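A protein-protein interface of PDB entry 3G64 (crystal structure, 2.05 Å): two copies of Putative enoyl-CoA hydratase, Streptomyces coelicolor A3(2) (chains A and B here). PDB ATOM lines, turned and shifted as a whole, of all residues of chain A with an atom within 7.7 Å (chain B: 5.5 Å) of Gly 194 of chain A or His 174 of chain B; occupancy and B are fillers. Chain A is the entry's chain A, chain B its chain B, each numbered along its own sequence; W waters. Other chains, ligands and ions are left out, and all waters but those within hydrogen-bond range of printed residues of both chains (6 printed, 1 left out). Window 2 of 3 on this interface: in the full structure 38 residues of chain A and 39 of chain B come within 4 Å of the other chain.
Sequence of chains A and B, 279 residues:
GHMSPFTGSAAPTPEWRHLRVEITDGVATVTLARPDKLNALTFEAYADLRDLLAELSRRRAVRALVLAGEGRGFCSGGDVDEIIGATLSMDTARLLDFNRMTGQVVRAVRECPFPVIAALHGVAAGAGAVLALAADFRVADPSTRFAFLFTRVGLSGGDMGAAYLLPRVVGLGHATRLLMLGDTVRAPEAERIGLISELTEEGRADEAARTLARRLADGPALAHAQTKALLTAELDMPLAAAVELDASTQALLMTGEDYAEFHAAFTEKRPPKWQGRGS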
ATOM      1  N   LEU A 133     -32.828  26.868 -12.017  1.00  0.00           N
ATOM      2  CA  LEU A 133     -32.041  26.683 -13.233  1.00  0.00           C
ATOM      3  C   LEU A 133     -32.226  27.857 -14.217  1.00  0.00           C
ATOM      4  O   LEU A 133     -31.312  28.206 -14.960  1.00  0.00           O
ATOM      5  CB  LEU A 133     -32.485  25.354 -13.887  1.00  0.00           C
ATOM      6  CG  LEU A 133     -31.775  24.827 -15.134  1.00  0.00           C
ATOM      7  CD1 LEU A 133     -30.305  24.535 -14.798  1.00  0.00           C
ATOM      8  CD2 LEU A 133     -32.498  23.569 -15.625  1.00  0.00           C
ATOM      9  N   ASP A 136     -30.321  33.690 -13.627  1.00  0.00           N
ATOM     10  CA  ASP A 136     -29.002  33.975 -14.150  1.00  0.00           C
ATOM     11  C   ASP A 136     -27.921  33.507 -13.183  1.00  0.00           C
ATOM     12  O   ASP A 136     -26.844  33.034 -13.620  1.00  0.00           O
ATOM     13  CB  ASP A 136     -28.900  35.471 -14.443  1.00  0.00           C
ATOM     14  CG  ASP A 136     -30.009  35.918 -15.404  1.00  0.00           C
ATOM     15  OD1 ASP A 136     -29.919  35.547 -16.596  1.00  0.00           O
ATOM     16  OD2 ASP A 136     -30.988  36.564 -14.962  1.00  0.00           O
ATOM     17  N   PHE A 137     -28.211  33.621 -11.878  1.00  0.00           N
ATOM     18  CA  PHE A 137     -27.257  33.234 -10.831  1.00  0.00           C
ATOM     19  C   PHE A 137     -27.935  32.322  -9.816  1.00  0.00           C
ATOM     20  O   PHE A 137     -29.085  32.565  -9.430  1.00  0.00           O
ATOM     21  CB  PHE A 137     -26.664  34.455 -10.093  1.00  0.00           C
ATOM     22  CG  PHE A 137     -25.885  35.405 -10.970  1.00  0.00           C
ATOM     23  CD1 PHE A 137     -24.499  35.320 -11.054  1.00  0.00           C
ATOM     24  CD2 PHE A 137     -26.537  36.388 -11.691  1.00  0.00           C
ATOM     25  CE1 PHE A 137     -23.780  36.200 -11.855  1.00  0.00           C
ATOM     26  CE2 PHE A 137     -25.826  37.280 -12.517  1.00  0.00           C
ATOM     27  CZ  PHE A 137     -24.447  37.181 -12.595  1.00  0.00           C
ATOM     28  N   ARG A 138     -27.214  31.275  -9.394  1.00  0.00           N
ATOM     29  CA  ARG A 138     -27.625  30.425  -8.275  1.00  0.00           C
ATOM     30  C   ARG A 138     -26.599  30.561  -7.128  1.00  0.00           C
ATOM     31  O   ARG A 138     -25.455  30.090  -7.216  1.00  0.00           O
ATOM     32  CB  ARG A 138     -27.778  28.961  -8.703  1.00  0.00           C
ATOM     33  CG  ARG A 138     -29.065  28.675  -9.561  1.00  0.00           C
ATOM     34  CD  ARG A 138     -28.893  27.460 -10.495  1.00  0.00           C
ATOM     35  NE  ARG A 138     -27.852  27.756 -11.470  1.00  0.00           N
ATOM     36  CZ  ARG A 138     -28.006  28.586 -12.506  1.00  0.00           C
ATOM     37  NH1 ARG A 138     -26.977  28.837 -13.303  1.00  0.00           N
ATOM     38  NH2 ARG A 138     -29.180  29.167 -12.755  1.00  0.00           N
ATOM     39  N   ARG A 168     -27.929  22.672 -21.510  1.00  0.00           N
ATOM     40  CA  ARG A 168     -27.137  23.853 -21.862  1.00  0.00           C
ATOM     41  C   ARG A 168     -26.334  24.381 -20.665  1.00  0.00           C
ATOM     42  O   ARG A 168     -25.395  25.171 -20.838  1.00  0.00           O
ATOM     43  CB  ARG A 168     -28.028  24.961 -22.448  1.00  0.00           C
ATOM     44  CG  ARG A 168     -28.460  24.600 -23.885  1.00  0.00           C
ATOM     45  CD  ARG A 168     -29.657  25.396 -24.326  1.00  0.00           C
ATOM     46  NE  ARG A 168     -29.952  25.156 -25.749  1.00  0.00           N
ATOM     47  CZ  ARG A 168     -30.700  24.152 -26.220  1.00  0.00           C
ATOM     48  NH1 ARG A 168     -31.212  23.247 -25.390  1.00  0.00           N
ATOM     49  NH2 ARG A 168     -30.931  24.054 -27.542  1.00  0.00           N
ATOM     50  N   VAL A 169     -26.687  23.920 -19.467  1.00  0.00           N
ATOM     51  CA  VAL A 169     -25.945  24.316 -18.266  1.00  0.00           C
ATOM     52  C   VAL A 169     -24.909  23.254 -17.896  1.00  0.00           C
ATOM     53  O   VAL A 169     -23.762  23.581 -17.617  1.00  0.00           O
ATOM     54  CB  VAL A 169     -26.907  24.605 -17.075  1.00  0.00           C
ATOM     55  CG1 VAL A 169     -26.125  24.883 -15.779  1.00  0.00           C
ATOM     56  CG2 VAL A 169     -27.804  25.802 -17.414  1.00  0.00           C
ATOM     57  N   VAL A 170     -25.299  21.983 -17.911  1.00  0.00           N
ATOM     58  CA  VAL A 170     -24.441  20.936 -17.370  1.00  0.00           C
ATOM     59  C   VAL A 170     -23.964  19.911 -18.398  1.00  0.00           C
ATOM     60  O   VAL A 170     -23.240  18.988 -18.043  1.00  0.00           O
ATOM     61  CB  VAL A 170     -25.124  20.190 -16.182  1.00  0.00           C
ATOM     62  CG1 VAL A 170     -25.506  21.171 -15.070  1.00  0.00           C
ATOM     63  CG2 VAL A 170     -26.381  19.375 -16.656  1.00  0.00           C
ATOM     64  N   HIS A 174     -24.994  14.570 -18.232  1.00  0.00           N
ATOM     65  CA  HIS A 174     -25.518  14.838 -16.880  1.00  0.00           C
ATOM     66  C   HIS A 174     -27.006  15.196 -16.939  1.00  0.00           C
ATOM     67  O   HIS A 174     -27.779  14.790 -16.069  1.00  0.00           O
ATOM     68  CB  HIS A 174     -24.770  16.005 -16.218  1.00  0.00           C
ATOM     69  CG  HIS A 174     -23.325  15.714 -15.888  1.00  0.00           C
ATOM     70  ND1 HIS A 174     -22.923  14.559 -15.270  1.00  0.00           N
ATOM     71  CD2 HIS A 174     -22.213  16.479 -16.033  1.00  0.00           C
ATOM     72  CE1 HIS A 174     -21.604  14.597 -15.073  1.00  0.00           C
ATOM     73  NE2 HIS A 174     -21.158  15.752 -15.510  1.00  0.00           N
ATOM     74  N   PRO A 188     -21.928  19.551  -3.541  1.00  0.00           N
ATOM     75  CA  PRO A 188     -20.619  19.347  -4.185  1.00  0.00           C
ATOM     76  C   PRO A 188     -20.746  18.893  -5.647  1.00  0.00           C
ATOM     77  O   PRO A 188     -20.036  19.387  -6.507  1.00  0.00           O
ATOM     78  CB  PRO A 188     -19.955  18.253  -3.322  1.00  0.00           C
ATOM     79  CG  PRO A 188     -20.685  18.302  -1.990  1.00  0.00           C
ATOM     80  CD  PRO A 188     -22.117  18.686  -2.362  1.00  0.00           C
ATOM     81  N   GLU A 189     -21.652  17.964  -5.916  1.00  0.00           N
ATOM     82  CA  GLU A 189     -21.870  17.520  -7.276  1.00  0.00           C
ATOM     83  C   GLU A 189     -22.402  18.689  -8.124  1.00  0.00           C
ATOM     84  O   GLU A 189     -21.943  18.914  -9.242  1.00  0.00           O
ATOM     85  CB  GLU A 189     -22.868  16.358  -7.306  1.00  0.00           C
ATOM     86  CG  GLU A 189     -23.183  15.934  -8.743  1.00  0.00           C
ATOM     87  CD  GLU A 189     -24.138  14.764  -8.856  1.00  0.00           C
ATOM     88  OE1 GLU A 189     -24.685  14.294  -7.831  1.00  0.00           O
ATOM     89  OE2 GLU A 189     -24.359  14.322  -9.996  1.00  0.00           O
ATOM     90  N   ALA A 190     -23.371  19.418  -7.571  1.00  0.00           N
ATOM     91  CA  ALA A 190     -23.973  20.576  -8.239  1.00  0.00           C
ATOM     92  C   ALA A 190     -22.899  21.588  -8.633  1.00  0.00           C
ATOM     93  O   ALA A 190     -22.900  22.097  -9.760  1.00  0.00           O
ATOM     94  CB  ALA A 190     -25.040  21.230  -7.339  1.00  0.00           C
ATOM     95  N   GLU A 191     -21.981  21.868  -7.707  1.00  0.00           N
ATOM     96  CA  GLU A 191     -20.868  22.761  -7.988  1.00  0.00           C
ATOM     97  C   GLU A 191     -19.966  22.202  -9.094  1.00  0.00           C
ATOM     98  O   GLU A 191     -19.599  22.909 -10.018  1.00  0.00           O
ATOM     99  CB  GLU A 191     -20.060  22.992  -6.706  1.00  0.00           C
ATOM    100  CG  GLU A 191     -19.316  24.309  -6.676  1.00  0.00           C
ATOM    101  CD  GLU A 191     -18.136  24.354  -7.629  1.00  0.00           C
ATOM    102  OE1 GLU A 191     -17.391  23.347  -7.722  1.00  0.00           O
ATOM    103  OE2 GLU A 191     -17.943  25.407  -8.282  1.00  0.00           O
ATOM    104  N   ARG A 192     -19.579  20.936  -8.974  1.00  0.00           N
ATOM    105  CA  ARG A 192     -18.759  20.291 -10.000  1.00  0.00           C
ATOM    106  C   ARG A 192     -19.387  20.351 -11.400  1.00  0.00           C
ATOM    107  O   ARG A 192     -18.699  20.626 -12.381  1.00  0.00           O
ATOM    108  CB  ARG A 192     -18.498  18.818  -9.640  1.00  0.00           C
ATOM    109  CG  ARG A 192     -17.530  18.608  -8.460  1.00  0.00           C
ATOM    110  CD  ARG A 192     -17.011  17.151  -8.389  1.00  0.00           C
ATOM    111  NE  ARG A 192     -18.070  16.134  -8.449  1.00  0.00           N
ATOM    112  CZ  ARG A 192     -18.699  15.635  -7.387  1.00  0.00           C
ATOM    113  NH1 ARG A 192     -18.408  16.059  -6.172  1.00  0.00           N
ATOM    114  NH2 ARG A 192     -19.625  14.711  -7.541  1.00  0.00           N
ATOM    115  N   ILE A 193     -20.679  20.069 -11.518  1.00  0.00           N
ATOM    116  CA  ILE A 193     -21.262  19.987 -12.855  1.00  0.00           C
ATOM    117  C   ILE A 193     -21.723  21.323 -13.427  1.00  0.00           C
ATOM    118  O   ILE A 193     -22.218  21.369 -14.562  1.00  0.00           O
ATOM    119  CB  ILE A 193     -22.372  18.907 -12.984  1.00  0.00           C
ATOM    120  CG1 ILE A 193     -23.667  19.335 -12.290  1.00  0.00           C
ATOM    121  CG2 ILE A 193     -21.883  17.534 -12.475  1.00  0.00           C
ATOM    122  CD1 ILE A 193     -24.735  18.219 -12.234  1.00  0.00           C
ATOM    123  N   GLY A 194     -21.580  22.410 -12.670  1.00  0.00           N
ATOM    124  CA  GLY A 194     -21.910  23.721 -13.226  1.00  0.00           C
ATOM    125  C   GLY A 194     -23.222  24.390 -12.816  1.00  0.00           C
ATOM    126  O   GLY A 194     -23.611  25.419 -13.395  1.00  0.00           O
ATOM    127  N   LEU A 195     -23.883  23.843 -11.804  1.00  0.00           N
ATOM    128  CA  LEU A 195     -25.173  24.387 -11.351  1.00  0.00           C
ATOM    129  C   LEU A 195     -25.081  25.505 -10.321  1.00  0.00           C
ATOM    130  O   LEU A 195     -26.096  26.148 -10.045  1.00  0.00           O
ATOM    131  CB  LEU A 195     -26.041  23.297 -10.744  1.00  0.00           C
ATOM    132  CG  LEU A 195     -26.730  22.322 -11.672  1.00  0.00           C
ATOM    133  CD1 LEU A 195     -27.388  21.190 -10.843  1.00  0.00           C
ATOM    134  CD2 LEU A 195     -27.746  23.094 -12.493  1.00  0.00           C
ATOM    135  N   ILE A 196     -23.892  25.734  -9.749  1.00  0.00           N
ATOM    136  CA  ILE A 196     -23.732  26.761  -8.709  1.00  0.00           C
ATOM    137  C   ILE A 196     -22.893  27.934  -9.170  1.00  0.00           C
ATOM    138  O   ILE A 196     -21.774  27.735  -9.660  1.00  0.00           O
ATOM    139  CB  ILE A 196     -23.028  26.183  -7.461  1.00  0.00           C
ATOM    140  CG1 ILE A 196     -23.780  24.955  -6.956  1.00  0.00           C
ATOM    141  CG2 ILE A 196     -22.857  27.254  -6.353  1.00  0.00           C
ATOM    142  CD1 ILE A 196     -25.197  25.248  -6.638  1.00  0.00           C
ATOM    143  N   SER A 197     -23.400  29.156  -8.983  1.00  0.00           N
ATOM    144  CA  SER A 197     -22.639  30.360  -9.350  1.00  0.00           C
ATOM    145  C   SER A 197     -21.753  30.841  -8.196  1.00  0.00           C
ATOM    146  O   SER A 197     -20.666  31.368  -8.412  1.00  0.00           O
ATOM    147  CB  SER A 197     -23.597  31.487  -9.748  1.00  0.00           C
ATOM    148  OG  SER A 197     -24.625  30.984 -10.595  1.00  0.00           O
ATOM    149  N   LEU A 231     -26.906  36.483 -24.394  1.00  0.00           N
ATOM    150  CA  LEU A 231     -26.710  35.087 -24.002  1.00  0.00           C
ATOM    151  C   LEU A 231     -27.949  34.259 -24.364  1.00  0.00           C
ATOM    152  O   LEU A 231     -27.878  33.195 -24.990  1.00  0.00           O
ATOM    153  CB  LEU A 231     -26.469  34.992 -22.483  1.00  0.00           C
ATOM    154  CG  LEU A 231     -25.031  35.289 -22.061  1.00  0.00           C
ATOM    155  CD1 LEU A 231     -24.943  35.616 -20.550  1.00  0.00           C
ATOM    156  CD2 LEU A 231     -24.108  34.139 -22.465  1.00  0.00           C
ATOM    157  N   LEU B 166     -18.936  31.329 -25.392  1.00  0.00           N
ATOM    158  CA  LEU B 166     -18.627  30.932 -24.012  1.00  0.00           C
ATOM    159  C   LEU B 166     -19.560  29.867 -23.435  1.00  0.00           C
ATOM    160  O   LEU B 166     -19.093  28.842 -22.900  1.00  0.00           O
ATOM    161  CB  LEU B 166     -18.518  32.160 -23.097  1.00  0.00           C
ATOM    162  CG  LEU B 166     -17.912  31.911 -21.713  1.00  0.00           C
ATOM    163  CD1 LEU B 166     -16.507  31.257 -21.834  1.00  0.00           C
ATOM    164  CD2 LEU B 166     -17.835  33.251 -20.964  1.00  0.00           C
ATOM    165  N   VAL B 170     -18.187  26.476 -21.799  1.00  0.00           N
ATOM    166  CA  VAL B 170     -18.199  26.230 -20.349  1.00  0.00           C
ATOM    167  C   VAL B 170     -19.582  26.048 -19.726  1.00  0.00           C
ATOM    168  O   VAL B 170     -19.699  25.795 -18.527  1.00  0.00           O
ATOM    169  CB  VAL B 170     -17.479  27.360 -19.576  1.00  0.00           C
ATOM    170  CG1 VAL B 170     -16.034  27.530 -20.091  1.00  0.00           C
ATOM    171  CG2 VAL B 170     -18.249  28.682 -19.678  1.00  0.00           C
ATOM    172  N   GLY B 171     -20.638  26.163 -20.523  1.00  0.00           N
ATOM    173  CA  GLY B 171     -21.985  25.978 -19.983  1.00  0.00           C
ATOM    174  C   GLY B 171     -22.609  27.330 -19.713  1.00  0.00           C
ATOM    175  O   GLY B 171     -21.909  28.297 -19.424  1.00  0.00           O
ATOM    176  N   LEU B 172     -23.926  27.415 -19.800  1.00  0.00           N
ATOM    177  CA  LEU B 172     -24.607  28.703 -19.604  1.00  0.00           C
ATOM    178  C   LEU B 172     -24.441  29.352 -18.197  1.00  0.00           C
ATOM    179  O   LEU B 172     -24.418  30.587 -18.092  1.00  0.00           O
ATOM    180  CB  LEU B 172     -26.100  28.531 -19.926  1.00  0.00           C
ATOM    181  CG  LEU B 172     -26.988  29.746 -19.683  1.00  0.00           C
ATOM    182  CD1 LEU B 172     -26.571  30.904 -20.653  1.00  0.00           C
ATOM    183  CD2 LEU B 172     -28.471  29.306 -19.886  1.00  0.00           C
ATOM    184  N   GLY B 173     -24.374  28.544 -17.132  1.00  0.00           N
ATOM    185  CA  GLY B 173     -24.285  29.066 -15.748  1.00  0.00           C
ATOM    186  C   GLY B 173     -22.937  29.777 -15.561  1.00  0.00           C
ATOM    187  O   GLY B 173     -22.868  30.976 -15.204  1.00  0.00           O
ATOM    188  N   HIS B 174     -21.855  29.071 -15.874  1.00  0.00           N
ATOM    189  CA  HIS B 174     -20.514  29.707 -15.856  1.00  0.00           C
ATOM    190  C   HIS B 174     -20.380  30.910 -16.812  1.00  0.00           C
ATOM    191  O   HIS B 174     -19.788  31.939 -16.454  1.00  0.00           O
ATOM    192  CB  HIS B 174     -19.417  28.673 -16.155  1.00  0.00           C
ATOM    193  CG  HIS B 174     -19.262  27.620 -15.088  1.00  0.00           C
ATOM    194  ND1 HIS B 174     -19.328  27.906 -13.738  1.00  0.00           N
ATOM    195  CD2 HIS B 174     -19.030  26.286 -15.178  1.00  0.00           C
ATOM    196  CE1 HIS B 174     -19.148  26.793 -13.043  1.00  0.00           C
ATOM    197  NE2 HIS B 174     -18.966  25.795 -13.893  1.00  0.00           N
ATOM    198  N   ALA B 175     -20.918  30.792 -18.027  1.00  0.00           N
ATOM    199  CA  ALA B 175     -20.816  31.879 -18.998  1.00  0.00           C
ATOM    200  C   ALA B 175     -21.516  33.146 -18.499  1.00  0.00           C
ATOM    201  O   ALA B 175     -21.008  34.255 -18.663  1.00  0.00           O
ATOM    202  CB  ALA B 175     -21.405  31.440 -20.396  1.00  0.00           C
ATOM    203  N   THR B 176     -22.683  32.978 -17.886  1.00  0.00           N
ATOM    204  CA  THR B 176     -23.429  34.132 -17.387  1.00  0.00           C
ATOM    205  C   THR B 176     -22.607  34.859 -16.318  1.00  0.00           C
ATOM    206  O   THR B 176     -22.431  36.082 -16.376  1.00  0.00           O
ATOM    207  CB  THR B 176     -24.785  33.714 -16.813  1.00  0.00           C
ATOM    208  OG1 THR B 176     -25.576  33.138 -17.869  1.00  0.00           O
ATOM    209  CG2 THR B 176     -25.512  34.913 -16.265  1.00  0.00           C
ATOM    210  N   ARG B 177     -22.096  34.092 -15.365  1.00  0.00           N
ATOM    211  CA  ARG B 177     -21.206  34.618 -14.308  1.00  0.00           C
ATOM    212  C   ARG B 177     -19.977  35.370 -14.886  1.00  0.00           C
ATOM    213  O   ARG B 177     -19.742  36.559 -14.585  1.00  0.00           O
ATOM    214  CB  ARG B 177     -20.785  33.448 -13.396  1.00  0.00           C
ATOM    215  CG  ARG B 177     -19.809  33.766 -12.264  1.00  0.00           C
ATOM    216  CD  ARG B 177     -19.665  32.577 -11.294  1.00  0.00           C
ATOM    217  NE  ARG B 177     -19.134  31.361 -11.922  1.00  0.00           N
ATOM    218  CZ  ARG B 177     -17.831  31.125 -12.110  1.00  0.00           C
ATOM    219  NH1 ARG B 177     -16.926  32.035 -11.751  1.00  0.00           N
ATOM    220  NH2 ARG B 177     -17.415  30.005 -12.694  1.00  0.00           N
ATOM    221  N   LEU B 178     -19.216  34.687 -15.741  1.00  0.00           N
ATOM    222  CA  LEU B 178     -18.023  35.261 -16.352  1.00  0.00           C
ATOM    223  C   LEU B 178     -18.313  36.552 -17.138  1.00  0.00           C
ATOM    224  O   LEU B 178     -17.606  37.552 -16.993  1.00  0.00           O
ATOM    225  CB  LEU B 178     -17.339  34.230 -17.279  1.00  0.00           C
ATOM    226  CG  LEU B 178     -16.221  33.357 -16.657  1.00  0.00           C
ATOM    227  CD1 LEU B 178     -16.660  32.747 -15.337  1.00  0.00           C
ATOM    228  CD2 LEU B 178     -15.751  32.264 -17.595  1.00  0.00           C
ATOM    229  N   LEU B 179     -19.366  36.538 -17.953  1.00  0.00           N
ATOM    230  CA  LEU B 179     -19.588  37.650 -18.875  1.00  0.00           C
ATOM    231  C   LEU B 179     -20.289  38.779 -18.163  1.00  0.00           C
ATOM    232  O   LEU B 179     -20.140  39.930 -18.515  1.00  0.00           O
ATOM    233  CB  LEU B 179     -20.420  37.223 -20.108  1.00  0.00           C
ATOM    234  CG  LEU B 179     -19.731  36.309 -21.129  1.00  0.00           C
ATOM    235  CD1 LEU B 179     -20.652  35.948 -22.271  1.00  0.00           C
ATOM    236  CD2 LEU B 179     -18.506  36.977 -21.662  1.00  0.00           C
ATOM    237  N   ILE B 193     -13.489  24.348 -15.618  1.00  0.00           N
ATOM    238  CA  ILE B 193     -14.675  24.659 -16.378  1.00  0.00           C
ATOM    239  C   ILE B 193     -14.551  24.433 -17.886  1.00  0.00           C
ATOM    240  O   ILE B 193     -15.534  24.588 -18.604  1.00  0.00           O
ATOM    241  CB  ILE B 193     -15.207  26.079 -16.062  1.00  0.00           C
ATOM    242  CG1 ILE B 193     -14.306  27.148 -16.676  1.00  0.00           C
ATOM    243  CG2 ILE B 193     -15.410  26.244 -14.551  1.00  0.00           C
ATOM    244  CD1 ILE B 193     -14.802  28.558 -16.414  1.00  0.00           C
HETATM  245  O   HOH W   1     -28.059  34.610 -18.439  1.00  0.00           O
HETATM  246  O   HOH W   2     -24.221  31.974 -13.115  1.00  0.00           O
HETATM  247  O   HOH W   3     -22.874  26.313 -16.161  1.00  0.00           O
HETATM  248  O   HOH W   4     -17.825  23.383 -12.516  1.00  0.00           O
HETATM  249  O   HOH W   5     -18.590  22.572 -15.074  1.00  0.00           O
HETATM  250  O   HOH W   6     -21.379  29.188 -12.276  1.00  0.00           O
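Positions printed for both chains: 170, 174 and 193.
Water W2 lies within hydrogen-bond range of the backbone carbonyl oxygen (O) of Gly 173 of chain B (2.7 Å), the side-chain hydroxyl (OG) of Ser 197 of chain A (2.7 Å) and the backbone carbonyl oxygen (O) of Asp 136 of chain A (2.9 Å). Water W1 lies within hydrogen-bond range of OD1 of Asp 136 of chain A and OG1 of Thr 176 of chain B. Water W6 lies within hydrogen-bond range of a ring nitrogen (ND1) of His 174 of chain B (2.8 Å), the backbone carbonyl oxygen (O) of Ile 196 of chain A (3.0 Å) and the guanidinium group (NE) of Arg 177 of chain B (3.1 Å). Water W3 lies within hydrogen-bond range of the backbone NH (N) of Gly 173 of chain B, the backbone NH (N) of His 174 of chain B, the backbone carbonyl oxygen (O) of Gly 194 of chain A and the backbone carbonyl oxygen (O) of Val 169 of chain A. Water W4 lies within hydrogen-bond range of O of Arg 192 of chain A, NE2 of His 174 of chain B and O of Glu 191 of chain A. Water W5 lies within hydrogen-bond range of the backbone carbonyl oxygen of Arg 192 of chain A and a ring nitrogen (NE2) of His 174 of chain B.
Leu 133 of chain A touches none of the printed residues of chain B. Of the printed residues of chain B, Asp 136 of chain A touches Thr 176. Of the printed residues of chain B, Arg 138 of chain A touches Gly 173 (3.6 Å). Of the printed residues of chain B, Arg 168 of chain A touches Gly 171 and Leu 172. Gly 194 of chain A touches just one residue of chain B: His 174. Printed residues of chain B within 4 Å of Ser 197 of chain A: Arg 177. Of the printed residues of chain A, Gly 171 of chain B touches Arg 168 and Val 169. Gly 173 of chain B touches just one residue of chain A: Arg 138. The nearest residue of chain A that does not touch His 174 of chain B is Ile 196 of chain A (4.4 Å). The nearest printed residue of chain B that does not touch Leu 231 of chain A is Ala 175 of chain B (4.3 Å).
O of Arg 138 of chain A is in hydrogen-bond range of N of Ser 197 of chain A, 2.9 Å away. The backbone carbonyl oxygen (O) of Leu 133 of chain A is in hydrogen-bond range of the guanidinium group (NH2) of Arg 138 of chain A, 3.2 Å away. A ring nitrogen (ND1) of His 174 of chain B lies within hydrogen-bond range of the guanidinium group (NH2) of Arg 177 of chain B (3.0 Å). The backbone carbonyl oxygen of Leu 195 of chain A lies within hydrogen-bond range of the guanidinium group of Arg 138 of chain A (2.8 Å). O of Leu 172 of chain B sits at hydrogen-bond distance from OG1 of Thr 176 of chain B.
The backbone carbonyl oxygen of Arg 168 of chain A is in hydrogen-bond range of the backbone NH of Leu 172 of chain B, 2.9 Å away.
Of the 19 printed residues of chain A, 8 touch a printed residue of chain B. Printed residues of chain A that touch a printed residue of chain B: Asp 136, Phe 137, Arg 138, Arg 168, Val 169, Gly 194, Ser 197 and Leu 231. Hydrophobic or aromatic side chains of chain A that line the printed part of chain B: Phe 137 and Leu 231. Of the 12 printed residues of chain B, 7 touch a printed residue of chain A. Hydrophobic or aromatic side chains of chain B within 4 Å of the printed part of chain A: Leu 172, His 174 and Leu 179.
Asp 136 of chain A touches Thr 176 of chain B (O to CG2, 3.5 Å). CA of Arg 177 of chain B touches CE1 of Phe 137 of chain A, at 3.9 Å. Arg 138 of chain A touches Gly 173 of chain B. CA of Gly 171 of chain B touches O of Arg 168 of chain A, 3.6 Å away. Val 169 of chain A touches Gly 171 of chain B (O to CA, 3.8 Å). NE2 of His 174 of chain B touches CA of Gly 194 of chain A, at 3.7 Å. Arg 177 of chain B touches Ser 197 of chain A (CD to O, 3.3 Å). Leu 231 of chain A touches Thr 176 of chain B. CD2 of Leu 231 of chain A touches CD1 of Leu 179 of chain B, 3.9 Å away.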
